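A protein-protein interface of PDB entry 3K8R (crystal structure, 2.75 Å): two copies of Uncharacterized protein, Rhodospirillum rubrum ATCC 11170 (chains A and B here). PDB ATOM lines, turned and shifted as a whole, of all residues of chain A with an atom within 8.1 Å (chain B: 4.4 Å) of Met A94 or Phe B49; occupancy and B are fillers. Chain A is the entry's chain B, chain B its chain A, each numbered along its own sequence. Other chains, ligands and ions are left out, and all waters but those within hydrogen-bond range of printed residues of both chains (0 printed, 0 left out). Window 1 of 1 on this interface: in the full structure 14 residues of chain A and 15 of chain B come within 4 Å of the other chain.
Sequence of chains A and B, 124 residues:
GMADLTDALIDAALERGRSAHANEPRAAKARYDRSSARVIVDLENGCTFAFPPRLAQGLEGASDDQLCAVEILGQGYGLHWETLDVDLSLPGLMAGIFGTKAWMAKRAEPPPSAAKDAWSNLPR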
ATOM      1  N   GLU A  24      19.118 -12.826 -16.484  1.00  0.00           N
ATOM      2  CA  GLU A  24      18.757 -12.962 -17.892  1.00  0.00           C
ATOM      3  C   GLU A  24      18.579 -14.423 -18.333  1.00  0.00           C
ATOM      4  O   GLU A  24      19.221 -15.317 -17.775  1.00  0.00           O
ATOM      5  CB  GLU A  24      19.909 -12.352 -18.702  1.00  0.00           C
ATOM      6  CG  GLU A  24      19.540 -11.734 -20.049  1.00  0.00           C
ATOM      7  CD  GLU A  24      18.814 -10.397 -19.901  1.00  0.00           C
ATOM      8  OE1 GLU A  24      19.021  -9.704 -18.875  1.00  0.00           O
ATOM      9  OE2 GLU A  24      18.056 -10.024 -20.822  1.00  0.00           O
ATOM     10  N   PRO A  25      17.706 -14.676 -19.330  1.00  0.00           N
ATOM     11  CA  PRO A  25      17.605 -16.036 -19.850  1.00  0.00           C
ATOM     12  C   PRO A  25      18.863 -16.325 -20.653  1.00  0.00           C
ATOM     13  O   PRO A  25      19.361 -15.442 -21.355  1.00  0.00           O
ATOM     14  CB  PRO A  25      16.400 -15.966 -20.777  1.00  0.00           C
ATOM     15  CG  PRO A  25      16.359 -14.527 -21.210  1.00  0.00           C
ATOM     16  CD  PRO A  25      16.714 -13.789 -19.963  1.00  0.00           C
ATOM     17  N   ARG A  26      19.358 -17.551 -20.577  1.00  0.00           N
ATOM     18  CA  ARG A  26      20.616 -17.879 -21.210  1.00  0.00           C
ATOM     19  C   ARG A  26      20.533 -19.252 -21.887  1.00  0.00           C
ATOM     20  O   ARG A  26      20.107 -20.225 -21.273  1.00  0.00           O
ATOM     21  CB  ARG A  26      21.704 -17.806 -20.129  1.00  0.00           C
ATOM     22  CG  ARG A  26      23.064 -17.423 -20.666  1.00  0.00           C
ATOM     23  CD  ARG A  26      23.962 -16.719 -19.643  1.00  0.00           C
ATOM     24  NE  ARG A  26      24.764 -17.615 -18.814  1.00  0.00           N
ATOM     25  CZ  ARG A  26      24.394 -18.125 -17.642  1.00  0.00           C
ATOM     26  NH1 ARG A  26      23.195 -17.864 -17.131  1.00  0.00           N
ATOM     27  NH2 ARG A  26      25.237 -18.921 -16.981  1.00  0.00           N
ATOM     28  N   ALA A  27      20.937 -19.333 -23.150  1.00  0.00           N
ATOM     29  CA  ALA A  27      20.821 -20.586 -23.898  1.00  0.00           C
ATOM     30  C   ALA A  27      21.632 -21.738 -23.319  1.00  0.00           C
ATOM     31  O   ALA A  27      22.843 -21.638 -23.190  1.00  0.00           O
ATOM     32  CB  ALA A  27      21.204 -20.371 -25.358  1.00  0.00           C
ATOM     33  N   VAL A  41      15.767 -23.161 -29.092  1.00  0.00           N
ATOM     34  CA  VAL A  41      16.723 -22.838 -28.043  1.00  0.00           C
ATOM     35  C   VAL A  41      16.121 -23.167 -26.690  1.00  0.00           C
ATOM     36  O   VAL A  41      15.065 -22.634 -26.338  1.00  0.00           O
ATOM     37  CB  VAL A  41      17.083 -21.358 -28.031  1.00  0.00           C
ATOM     38  CG1 VAL A  41      18.153 -21.095 -26.973  1.00  0.00           C
ATOM     39  CG2 VAL A  41      17.570 -20.929 -29.393  1.00  0.00           C
ATOM     40  N   LEU A  43      16.351 -22.659 -22.989  1.00  0.00           N
ATOM     41  CA  LEU A  43      16.945 -21.742 -22.024  1.00  0.00           C
ATOM     42  C   LEU A  43      17.242 -22.439 -20.710  1.00  0.00           C
ATOM     43  O   LEU A  43      16.616 -23.441 -20.349  1.00  0.00           O
ATOM     44  CB  LEU A  43      16.053 -20.530 -21.797  1.00  0.00           C
ATOM     45  CG  LEU A  43      15.684 -19.771 -23.071  1.00  0.00           C
ATOM     46  CD1 LEU A  43      14.922 -18.534 -22.677  1.00  0.00           C
ATOM     47  CD2 LEU A  43      16.927 -19.418 -23.879  1.00  0.00           C
ATOM     48  N   ASN A  45      16.699 -21.580 -17.717  1.00  0.00           N
ATOM     49  CA  ASN A  45      15.701 -21.439 -16.664  1.00  0.00           C
ATOM     50  C   ASN A  45      14.462 -22.267 -16.935  1.00  0.00           C
ATOM     51  O   ASN A  45      13.433 -22.045 -16.306  1.00  0.00           O
ATOM     52  CB  ASN A  45      15.291 -19.974 -16.507  1.00  0.00           C
ATOM     53  CG  ASN A  45      14.671 -19.397 -17.769  1.00  0.00           C
ATOM     54  OD1 ASN A  45      14.283 -20.127 -18.679  1.00  0.00           O
ATOM     55  ND2 ASN A  45      14.589 -18.076 -17.830  1.00  0.00           N
ATOM     56  N   GLY A  46      14.545 -23.187 -17.891  1.00  0.00           N
ATOM     57  CA  GLY A  46      13.423 -24.063 -18.221  1.00  0.00           C
ATOM     58  C   GLY A  46      12.520 -23.571 -19.342  1.00  0.00           C
ATOM     59  O   GLY A  46      11.535 -24.230 -19.698  1.00  0.00           O
ATOM     60  N   CYS A  47      12.816 -22.408 -19.901  1.00  0.00           N
ATOM     61  CA  CYS A  47      11.998 -21.907 -21.002  1.00  0.00           C
ATOM     62  C   CYS A  47      12.605 -22.299 -22.332  1.00  0.00           C
ATOM     63  O   CYS A  47      13.776 -22.725 -22.401  1.00  0.00           O
ATOM     64  CB  CYS A  47      11.843 -20.404 -20.937  1.00  0.00           C
ATOM     65  SG  CYS A  47      10.897 -19.954 -19.543  1.00  0.00           S
ATOM     66  N   THR A  48      11.793 -22.156 -23.378  1.00  0.00           N
ATOM     67  CA  THR A  48      12.195 -22.496 -24.728  1.00  0.00           C
ATOM     68  C   THR A  48      11.796 -21.357 -25.660  1.00  0.00           C
ATOM     69  O   THR A  48      10.734 -20.730 -25.491  1.00  0.00           O
ATOM     70  CB  THR A  48      11.502 -23.804 -25.204  1.00  0.00           C
ATOM     71  OG1 THR A  48      11.603 -24.814 -24.189  1.00  0.00           O
ATOM     72  CG2 THR A  48      12.123 -24.316 -26.509  1.00  0.00           C
ATOM     73  N   PHE A  49      12.667 -21.082 -26.624  1.00  0.00           N
ATOM     74  CA  PHE A  49      12.422 -20.073 -27.641  1.00  0.00           C
ATOM     75  C   PHE A  49      12.746 -20.728 -28.966  1.00  0.00           C
ATOM     76  O   PHE A  49      13.743 -21.435 -29.085  1.00  0.00           O
ATOM     77  CB  PHE A  49      13.299 -18.844 -27.421  1.00  0.00           C
ATOM     78  CG  PHE A  49      13.108 -17.771 -28.454  1.00  0.00           C
ATOM     79  CD1 PHE A  49      11.994 -16.934 -28.409  1.00  0.00           C
ATOM     80  CD2 PHE A  49      14.044 -17.583 -29.458  1.00  0.00           C
ATOM     81  CE1 PHE A  49      11.803 -15.938 -29.356  1.00  0.00           C
ATOM     82  CE2 PHE A  49      13.865 -16.588 -30.416  1.00  0.00           C
ATOM     83  CZ  PHE A  49      12.739 -15.761 -30.359  1.00  0.00           C
ATOM     84  N   ALA A  50      11.878 -20.517 -29.947  1.00  0.00           N
ATOM     85  CA  ALA A  50      12.065 -21.093 -31.265  1.00  0.00           C
ATOM     86  C   ALA A  50      11.840 -20.002 -32.284  1.00  0.00           C
ATOM     87  O   ALA A  50      11.022 -19.115 -32.058  1.00  0.00           O
ATOM     88  CB  ALA A  50      11.086 -22.226 -31.485  1.00  0.00           C
ATOM     89  N   PHE A  51      12.572 -20.046 -33.394  1.00  0.00           N
ATOM     90  CA  PHE A  51      12.381 -19.062 -34.460  1.00  0.00           C
ATOM     91  C   PHE A  51      12.608 -19.691 -35.816  1.00  0.00           C
ATOM     92  O   PHE A  51      13.454 -20.576 -35.957  1.00  0.00           O
ATOM     93  CB  PHE A  51      13.278 -17.820 -34.274  1.00  0.00           C
ATOM     94  CG  PHE A  51      14.765 -18.091 -34.330  1.00  0.00           C
ATOM     95  CD1 PHE A  51      15.461 -18.486 -33.193  1.00  0.00           C
ATOM     96  CD2 PHE A  51      15.481 -17.894 -35.508  1.00  0.00           C
ATOM     97  CE1 PHE A  51      16.845 -18.720 -33.238  1.00  0.00           C
ATOM     98  CE2 PHE A  51      16.866 -18.124 -35.564  1.00  0.00           C
ATOM     99  CZ  PHE A  51      17.547 -18.537 -34.431  1.00  0.00           C
ATOM    100  N   SER A  89      22.129 -12.368 -31.603  1.00  0.00           N
ATOM    101  CA  SER A  89      21.914 -12.062 -30.190  1.00  0.00           C
ATOM    102  C   SER A  89      20.644 -12.725 -29.689  1.00  0.00           C
ATOM    103  O   SER A  89      19.558 -12.366 -30.138  1.00  0.00           O
ATOM    104  CB  SER A  89      21.765 -10.556 -30.008  1.00  0.00           C
ATOM    105  OG  SER A  89      21.364 -10.255 -28.688  1.00  0.00           O
ATOM    106  N   LEU A  90      20.738 -13.668 -28.755  1.00  0.00           N
ATOM    107  CA  LEU A  90      19.511 -14.327 -28.263  1.00  0.00           C
ATOM    108  C   LEU A  90      18.526 -13.290 -27.689  1.00  0.00           C
ATOM    109  O   LEU A  90      17.331 -13.312 -28.015  1.00  0.00           O
ATOM    110  CB  LEU A  90      19.823 -15.445 -27.260  1.00  0.00           C
ATOM    111  CG  LEU A  90      18.646 -16.202 -26.629  1.00  0.00           C
ATOM    112  CD1 LEU A  90      17.723 -16.858 -27.685  1.00  0.00           C
ATOM    113  CD2 LEU A  90      19.185 -17.246 -25.641  1.00  0.00           C
ATOM    114  N   PRO A  91      19.021 -12.364 -26.852  1.00  0.00           N
ATOM    115  CA  PRO A  91      18.122 -11.331 -26.345  1.00  0.00           C
ATOM    116  C   PRO A  91      17.494 -10.487 -27.464  1.00  0.00           C
ATOM    117  O   PRO A  91      16.328 -10.087 -27.353  1.00  0.00           O
ATOM    118  CB  PRO A  91      19.038 -10.465 -25.476  1.00  0.00           C
ATOM    119  CG  PRO A  91      20.120 -11.358 -25.065  1.00  0.00           C
ATOM    120  CD  PRO A  91      20.351 -12.285 -26.221  1.00  0.00           C
ATOM    121  N   GLY A  92      18.265 -10.204 -28.516  1.00  0.00           N
ATOM    122  CA  GLY A  92      17.768  -9.432 -29.657  1.00  0.00           C
ATOM    123  C   GLY A  92      16.652 -10.184 -30.355  1.00  0.00           C
ATOM    124  O   GLY A  92      15.590  -9.626 -30.625  1.00  0.00           O
ATOM    125  N   LEU A  93      16.900 -11.461 -30.631  1.00  0.00           N
ATOM    126  CA  LEU A  93      15.913 -12.330 -31.255  1.00  0.00           C
ATOM    127  C   LEU A  93      14.622 -12.382 -30.419  1.00  0.00           C
ATOM    128  O   LEU A  93      13.525 -12.227 -30.960  1.00  0.00           O
ATOM    129  CB  LEU A  93      16.495 -13.746 -31.463  1.00  0.00           C
ATOM    130  CG  LEU A  93      17.584 -13.892 -32.531  1.00  0.00           C
ATOM    131  CD1 LEU A  93      18.065 -15.325 -32.644  1.00  0.00           C
ATOM    132  CD2 LEU A  93      17.066 -13.406 -33.872  1.00  0.00           C
ATOM    133  N   MET A  94      14.758 -12.575 -29.105  1.00  0.00           N
ATOM    134  CA  MET A  94      13.589 -12.620 -28.202  1.00  0.00           C
ATOM    135  C   MET A  94      12.930 -11.253 -28.017  1.00  0.00           C
ATOM    136  O   MET A  94      11.776 -11.175 -27.623  1.00  0.00           O
ATOM    137  CB  MET A  94      13.957 -13.233 -26.852  1.00  0.00           C
ATOM    138  CG  MET A  94      14.388 -14.678 -26.998  1.00  0.00           C
ATOM    139  SD  MET A  94      14.848 -15.568 -25.370  1.00  0.00           S
ATOM    140  CE  MET A  94      13.199 -15.365 -24.377  1.00  0.00           C
ATOM    141  N   ALA A  95      13.665 -10.184 -28.304  1.00  0.00           N
ATOM    142  CA  ALA A  95      13.116  -8.837 -28.259  1.00  0.00           C
ATOM    143  C   ALA A  95      12.385  -8.539 -29.567  1.00  0.00           C
ATOM    144  O   ALA A  95      11.670  -7.544 -29.669  1.00  0.00           O
ATOM    145  CB  ALA A  95      14.219  -7.837 -28.047  1.00  0.00           C
ATOM    146  N   GLY A  96      12.569  -9.399 -30.568  1.00  0.00           N
ATOM    147  CA  GLY A  96      11.939  -9.223 -31.874  1.00  0.00           C
ATOM    148  C   GLY A  96      12.850  -8.585 -32.913  1.00  0.00           C
ATOM    149  O   GLY A  96      12.393  -8.253 -34.009  1.00  0.00           O
ATOM    150  N   ILE A  97      14.134  -8.419 -32.582  1.00  0.00           N
ATOM    151  CA  ILE A  97      15.102  -7.822 -33.494  1.00  0.00           C
ATOM    152  C   ILE A  97      15.843  -8.940 -34.224  1.00  0.00           C
ATOM    153  O   ILE A  97      16.619  -9.676 -33.617  1.00  0.00           O
ATOM    154  CB  ILE A  97      16.122  -6.931 -32.749  1.00  0.00           C
ATOM    155  CG1 ILE A  97      15.415  -5.981 -31.782  1.00  0.00           C
ATOM    156  CG2 ILE A  97      16.961  -6.138 -33.750  1.00  0.00           C
ATOM    157  CD1 ILE A  97      16.356  -5.116 -30.986  1.00  0.00           C
ATOM    158  N   PHE A  98      15.594  -9.063 -35.528  1.00  0.00           N
ATOM    159  CA  PHE A  98      16.207 -10.113 -36.355  1.00  0.00           C
ATOM    160  C   PHE A  98      17.239  -9.580 -37.334  1.00  0.00           C
ATOM    161  O   PHE A  98      17.802 -10.333 -38.126  1.00  0.00           O
ATOM    162  CB  PHE A  98      15.136 -10.827 -37.178  1.00  0.00           C
ATOM    163  CG  PHE A  98      13.995 -11.326 -36.371  1.00  0.00           C
ATOM    164  CD1 PHE A  98      14.126 -12.492 -35.627  1.00  0.00           C
ATOM    165  CD2 PHE A  98      12.786 -10.632 -36.356  1.00  0.00           C
ATOM    166  CE1 PHE A  98      13.072 -12.962 -34.871  1.00  0.00           C
ATOM    167  CE2 PHE A  98      11.725 -11.085 -35.608  1.00  0.00           C
ATOM    168  CZ  PHE A  98      11.859 -12.257 -34.859  1.00  0.00           C
ATOM    169  N   PRO B  25       7.602  -8.310 -29.463  1.00  0.00           N
ATOM    170  CA  PRO B  25       6.855  -9.558 -29.703  1.00  0.00           C
ATOM    171  C   PRO B  25       5.488  -9.522 -29.006  1.00  0.00           C
ATOM    172  O   PRO B  25       5.348  -8.903 -27.946  1.00  0.00           O
ATOM    173  CB  PRO B  25       7.744 -10.619 -29.059  1.00  0.00           C
ATOM    174  CG  PRO B  25       8.315  -9.932 -27.893  1.00  0.00           C
ATOM    175  CD  PRO B  25       8.507  -8.473 -28.306  1.00  0.00           C
ATOM    176  N   VAL B  39       3.357 -23.852 -21.002  1.00  0.00           N
ATOM    177  CA  VAL B  39       2.395 -22.994 -21.671  1.00  0.00           C
ATOM    178  C   VAL B  39       3.086 -22.588 -22.966  1.00  0.00           C
ATOM    179  O   VAL B  39       4.100 -21.903 -22.916  1.00  0.00           O
ATOM    180  CB  VAL B  39       2.076 -21.746 -20.852  1.00  0.00           C
ATOM    181  CG1 VAL B  39       1.125 -20.824 -21.622  1.00  0.00           C
ATOM    182  CG2 VAL B  39       1.494 -22.136 -19.503  1.00  0.00           C
ATOM    183  N   ILE B  40       2.583 -23.047 -24.115  1.00  0.00           N
ATOM    184  CA  ILE B  40       3.180 -22.697 -25.418  1.00  0.00           C
ATOM    185  C   ILE B  40       2.522 -21.433 -25.984  1.00  0.00           C
ATOM    186  O   ILE B  40       1.287 -21.381 -26.130  1.00  0.00           O
ATOM    187  CB  ILE B  40       3.067 -23.842 -26.444  1.00  0.00           C
ATOM    188  CG1 ILE B  40       3.715 -25.109 -25.888  1.00  0.00           C
ATOM    189  CG2 ILE B  40       3.746 -23.456 -27.742  1.00  0.00           C
ATOM    190  CD1 ILE B  40       3.611 -26.289 -26.803  1.00  0.00           C
ATOM    191  N   VAL B  41       3.354 -20.432 -26.294  1.00  0.00           N
ATOM    192  CA  VAL B  41       2.899 -19.140 -26.804  1.00  0.00           C
ATOM    193  C   VAL B  41       3.392 -18.893 -28.227  1.00  0.00           C
ATOM    194  O   VAL B  41       4.598 -18.808 -28.470  1.00  0.00           O
ATOM    195  CB  VAL B  41       3.408 -17.967 -25.939  1.00  0.00           C
ATOM    196  CG1 VAL B  41       2.772 -16.666 -26.407  1.00  0.00           C
ATOM    197  CG2 VAL B  41       3.108 -18.208 -24.470  1.00  0.00           C
ATOM    198  N   THR B  48       8.095 -18.708 -31.274  1.00  0.00           N
ATOM    199  CA  THR B  48       7.394 -19.461 -30.227  1.00  0.00           C
ATOM    200  C   THR B  48       8.139 -19.391 -28.903  1.00  0.00           C
ATOM    201  O   THR B  48       9.363 -19.562 -28.862  1.00  0.00           O
ATOM    202  CB  THR B  48       7.277 -20.945 -30.596  1.00  0.00           C
ATOM    203  OG1 THR B  48       6.880 -21.075 -31.959  1.00  0.00           O
ATOM    204  CG2 THR B  48       6.269 -21.651 -29.713  1.00  0.00           C
ATOM    205  N   PHE B  49       7.402 -19.147 -27.823  1.00  0.00           N
ATOM    206  CA  PHE B  49       7.974 -19.093 -26.477  1.00  0.00           C
ATOM    207  C   PHE B  49       7.228 -20.065 -25.570  1.00  0.00           C
ATOM    208  O   PHE B  49       6.004 -20.083 -25.560  1.00  0.00           O
ATOM    209  CB  PHE B  49       7.897 -17.671 -25.918  1.00  0.00           C
ATOM    210  CG  PHE B  49       8.376 -17.539 -24.492  1.00  0.00           C
ATOM    211  CD1 PHE B  49       9.732 -17.610 -24.191  1.00  0.00           C
ATOM    212  CD2 PHE B  49       7.480 -17.305 -23.467  1.00  0.00           C
ATOM    213  CE1 PHE B  49      10.180 -17.478 -22.891  1.00  0.00           C
ATOM    214  CE2 PHE B  49       7.919 -17.169 -22.165  1.00  0.00           C
ATOM    215  CZ  PHE B  49       9.279 -17.259 -21.878  1.00  0.00           C
ATOM    216  N   ALA B  50       7.970 -20.886 -24.832  1.00  0.00           N
ATOM    217  CA  ALA B  50       7.365 -21.847 -23.907  1.00  0.00           C
ATOM    218  C   ALA B  50       7.950 -21.624 -22.528  1.00  0.00           C
ATOM    219  O   ALA B  50       9.168 -21.492 -22.398  1.00  0.00           O
ATOM    220  CB  ALA B  50       7.623 -23.280 -24.362  1.00  0.00           C
ATOM    221  N   PHE B  51       7.092 -21.565 -21.510  1.00  0.00           N
ATOM    222  CA  PHE B  51       7.545 -21.427 -20.121  1.00  0.00           C
ATOM    223  C   PHE B  51       6.753 -22.370 -19.233  1.00  0.00           C
ATOM    224  O   PHE B  51       5.567 -22.607 -19.489  1.00  0.00           O
ATOM    225  CB  PHE B  51       7.374 -20.004 -19.624  1.00  0.00           C
ATOM    226  CG  PHE B  51       5.938 -19.563 -19.505  1.00  0.00           C
ATOM    227  CD1 PHE B  51       5.242 -19.099 -20.612  1.00  0.00           C
ATOM    228  CD2 PHE B  51       5.286 -19.588 -18.276  1.00  0.00           C
ATOM    229  CE1 PHE B  51       3.905 -18.680 -20.504  1.00  0.00           C
ATOM    230  CE2 PHE B  51       3.949 -19.170 -18.154  1.00  0.00           C
ATOM    231  CZ  PHE B  51       3.259 -18.714 -19.271  1.00  0.00           C
ATOM    232  N   LEU B  90       4.100 -11.038 -20.713  1.00  0.00           N
ATOM    233  CA  LEU B  90       4.862 -11.858 -21.682  1.00  0.00           C
ATOM    234  C   LEU B  90       6.308 -11.360 -21.775  1.00  0.00           C
ATOM    235  O   LEU B  90       7.254 -12.154 -21.660  1.00  0.00           O
ATOM    236  CB  LEU B  90       4.191 -11.871 -23.061  1.00  0.00           C
ATOM    237  CG  LEU B  90       4.892 -12.560 -24.234  1.00  0.00           C
ATOM    238  CD1 LEU B  90       5.185 -14.043 -23.949  1.00  0.00           C
ATOM    239  CD2 LEU B  90       4.027 -12.403 -25.477  1.00  0.00           C
ATOM    240  N   LEU B  93       8.128 -12.456 -18.683  1.00  0.00           N
ATOM    241  CA  LEU B  93       8.419 -13.886 -18.731  1.00  0.00           C
ATOM    242  C   LEU B  93       9.569 -14.169 -19.695  1.00  0.00           C
ATOM    243  O   LEU B  93      10.429 -14.994 -19.420  1.00  0.00           O
ATOM    244  CB  LEU B  93       7.171 -14.692 -19.136  1.00  0.00           C
ATOM    245  CG  LEU B  93       6.015 -14.796 -18.129  1.00  0.00           C
ATOM    246  CD1 LEU B  93       4.850 -15.565 -18.732  1.00  0.00           C
ATOM    247  CD2 LEU B  93       6.457 -15.461 -16.845  1.00  0.00           C
ATOM    248  N   MET B  94       9.597 -13.467 -20.823  1.00  0.00           N
ATOM    249  CA  MET B  94      10.665 -13.675 -21.802  1.00  0.00           C
ATOM    250  C   MET B  94      11.997 -13.093 -21.315  1.00  0.00           C
ATOM    251  O   MET B  94      13.055 -13.517 -21.757  1.00  0.00           O
ATOM    252  CB  MET B  94      10.247 -13.134 -23.177  1.00  0.00           C
ATOM    253  CG  MET B  94       9.002 -13.865 -23.708  1.00  0.00           C
ATOM    254  SD  MET B  94       8.508 -13.508 -25.547  1.00  0.00           S
ATOM    255  CE  MET B  94      10.058 -14.184 -26.475  1.00  0.00           C
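Of the printed residues of chain B, Pro A25 touches Met B94 (3.5 Å). Gly A92 touches none of the printed residues of chain B. Phe A98 touches none of the printed residues of chain B. Of the printed residues of chain A, Pro B25 touches Met A94 (3.7 Å) and Ala A95 (3.6 Å). Phe B49 touches just these residues of chain A: Cys A47, Thr A48 and Met A94. Printed residues of chain A within 4 Å of Met B94: Pro A25, Phe A49 and Met A94. The nearest printed residue of chain B that does not touch Met A94 is Leu B93 (5.7 Å). The nearest printed residue of chain B that does not touch Ala A50 is Phe B49 (5.1 Å).
N of Ala B50 lies within hydrogen-bond range of O of Thr A48 (2.8 Å). The backbone carbonyl oxygen (O) of Ala B50 lies close to the side-chain sulfur (SG) of Cys A47 (3.7 Å). O of Thr B48 sits at hydrogen-bond distance from N of Ala A50, 2.9 Å away.
Of the 11 printed residues of chain B, 6 touch a printed residue of chain A. Printed residues of chain A that touch a printed residue of chain B: Pro A25, Cys A47, Thr A48, Phe A49, Ala A50, Met A94 and Ala A95. Hydrophobic or aromatic side chains of chain A within 4 Å of the printed part of chain B: Pro A25, Phe A49 and Met A94. Among the printed residues, 14 pairs touch across the chains. Among the printed residues, no Asp or Glu carboxylate lies within 4 Å of a Lys or Arg side-chain nitrogen of the other chain.
Pro A25 touches Met B94, and with the chains exchanged Met A94 touches Pro B25. Thr A48 touches its own counterpart, Thr B48. Thr A48 touches Ala B50, and with the chains exchanged Ala A50 touches Thr B48. Met B94 touches its own counterpart, Met A94. Of the 14 pairs that touch across the chains among the printed residues, 10 have their exchanged pair printed and touching as well.
CG of Pro A25 touches O of Met B94 (3.5 Å). SG of Cys A47 touches CB of Phe B51, 3.5 Å away. Thr A48 touches Thr B48 (O to O, 3.8 Å). O of Thr A48 touches CA of Phe B49, 3.4 Å away. CA of Phe A49 touches O of Thr B48, at 3.3 Å. Phe A49 touches Met B94. Met A94 touches Pro B25 (O to CG, 3.7 Å). Met A94 touches Phe B49. CE of Met A94 touches O of Met B94 (3.2 Å). CD of Pro B25 touches O of Ala A95, at 3.6 Å.
The backbone NH (N) of Cys A47 is in hydrogen-bond range of the side-chain amide oxygen (OD1) of Asn A45, at 3.0 Å. The backbone NH (N) of Val A41 is in hydrogen-bond range of the backbone carbonyl oxygen (O) of Phe A49 (2.7 Å). The backbone NH (N) of Val B41 sits at hydrogen-bond distance from the backbone carbonyl oxygen (O) of Phe B49. O of Phe B51 is in hydrogen-bond range of N of Val B39 (3.0 Å).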
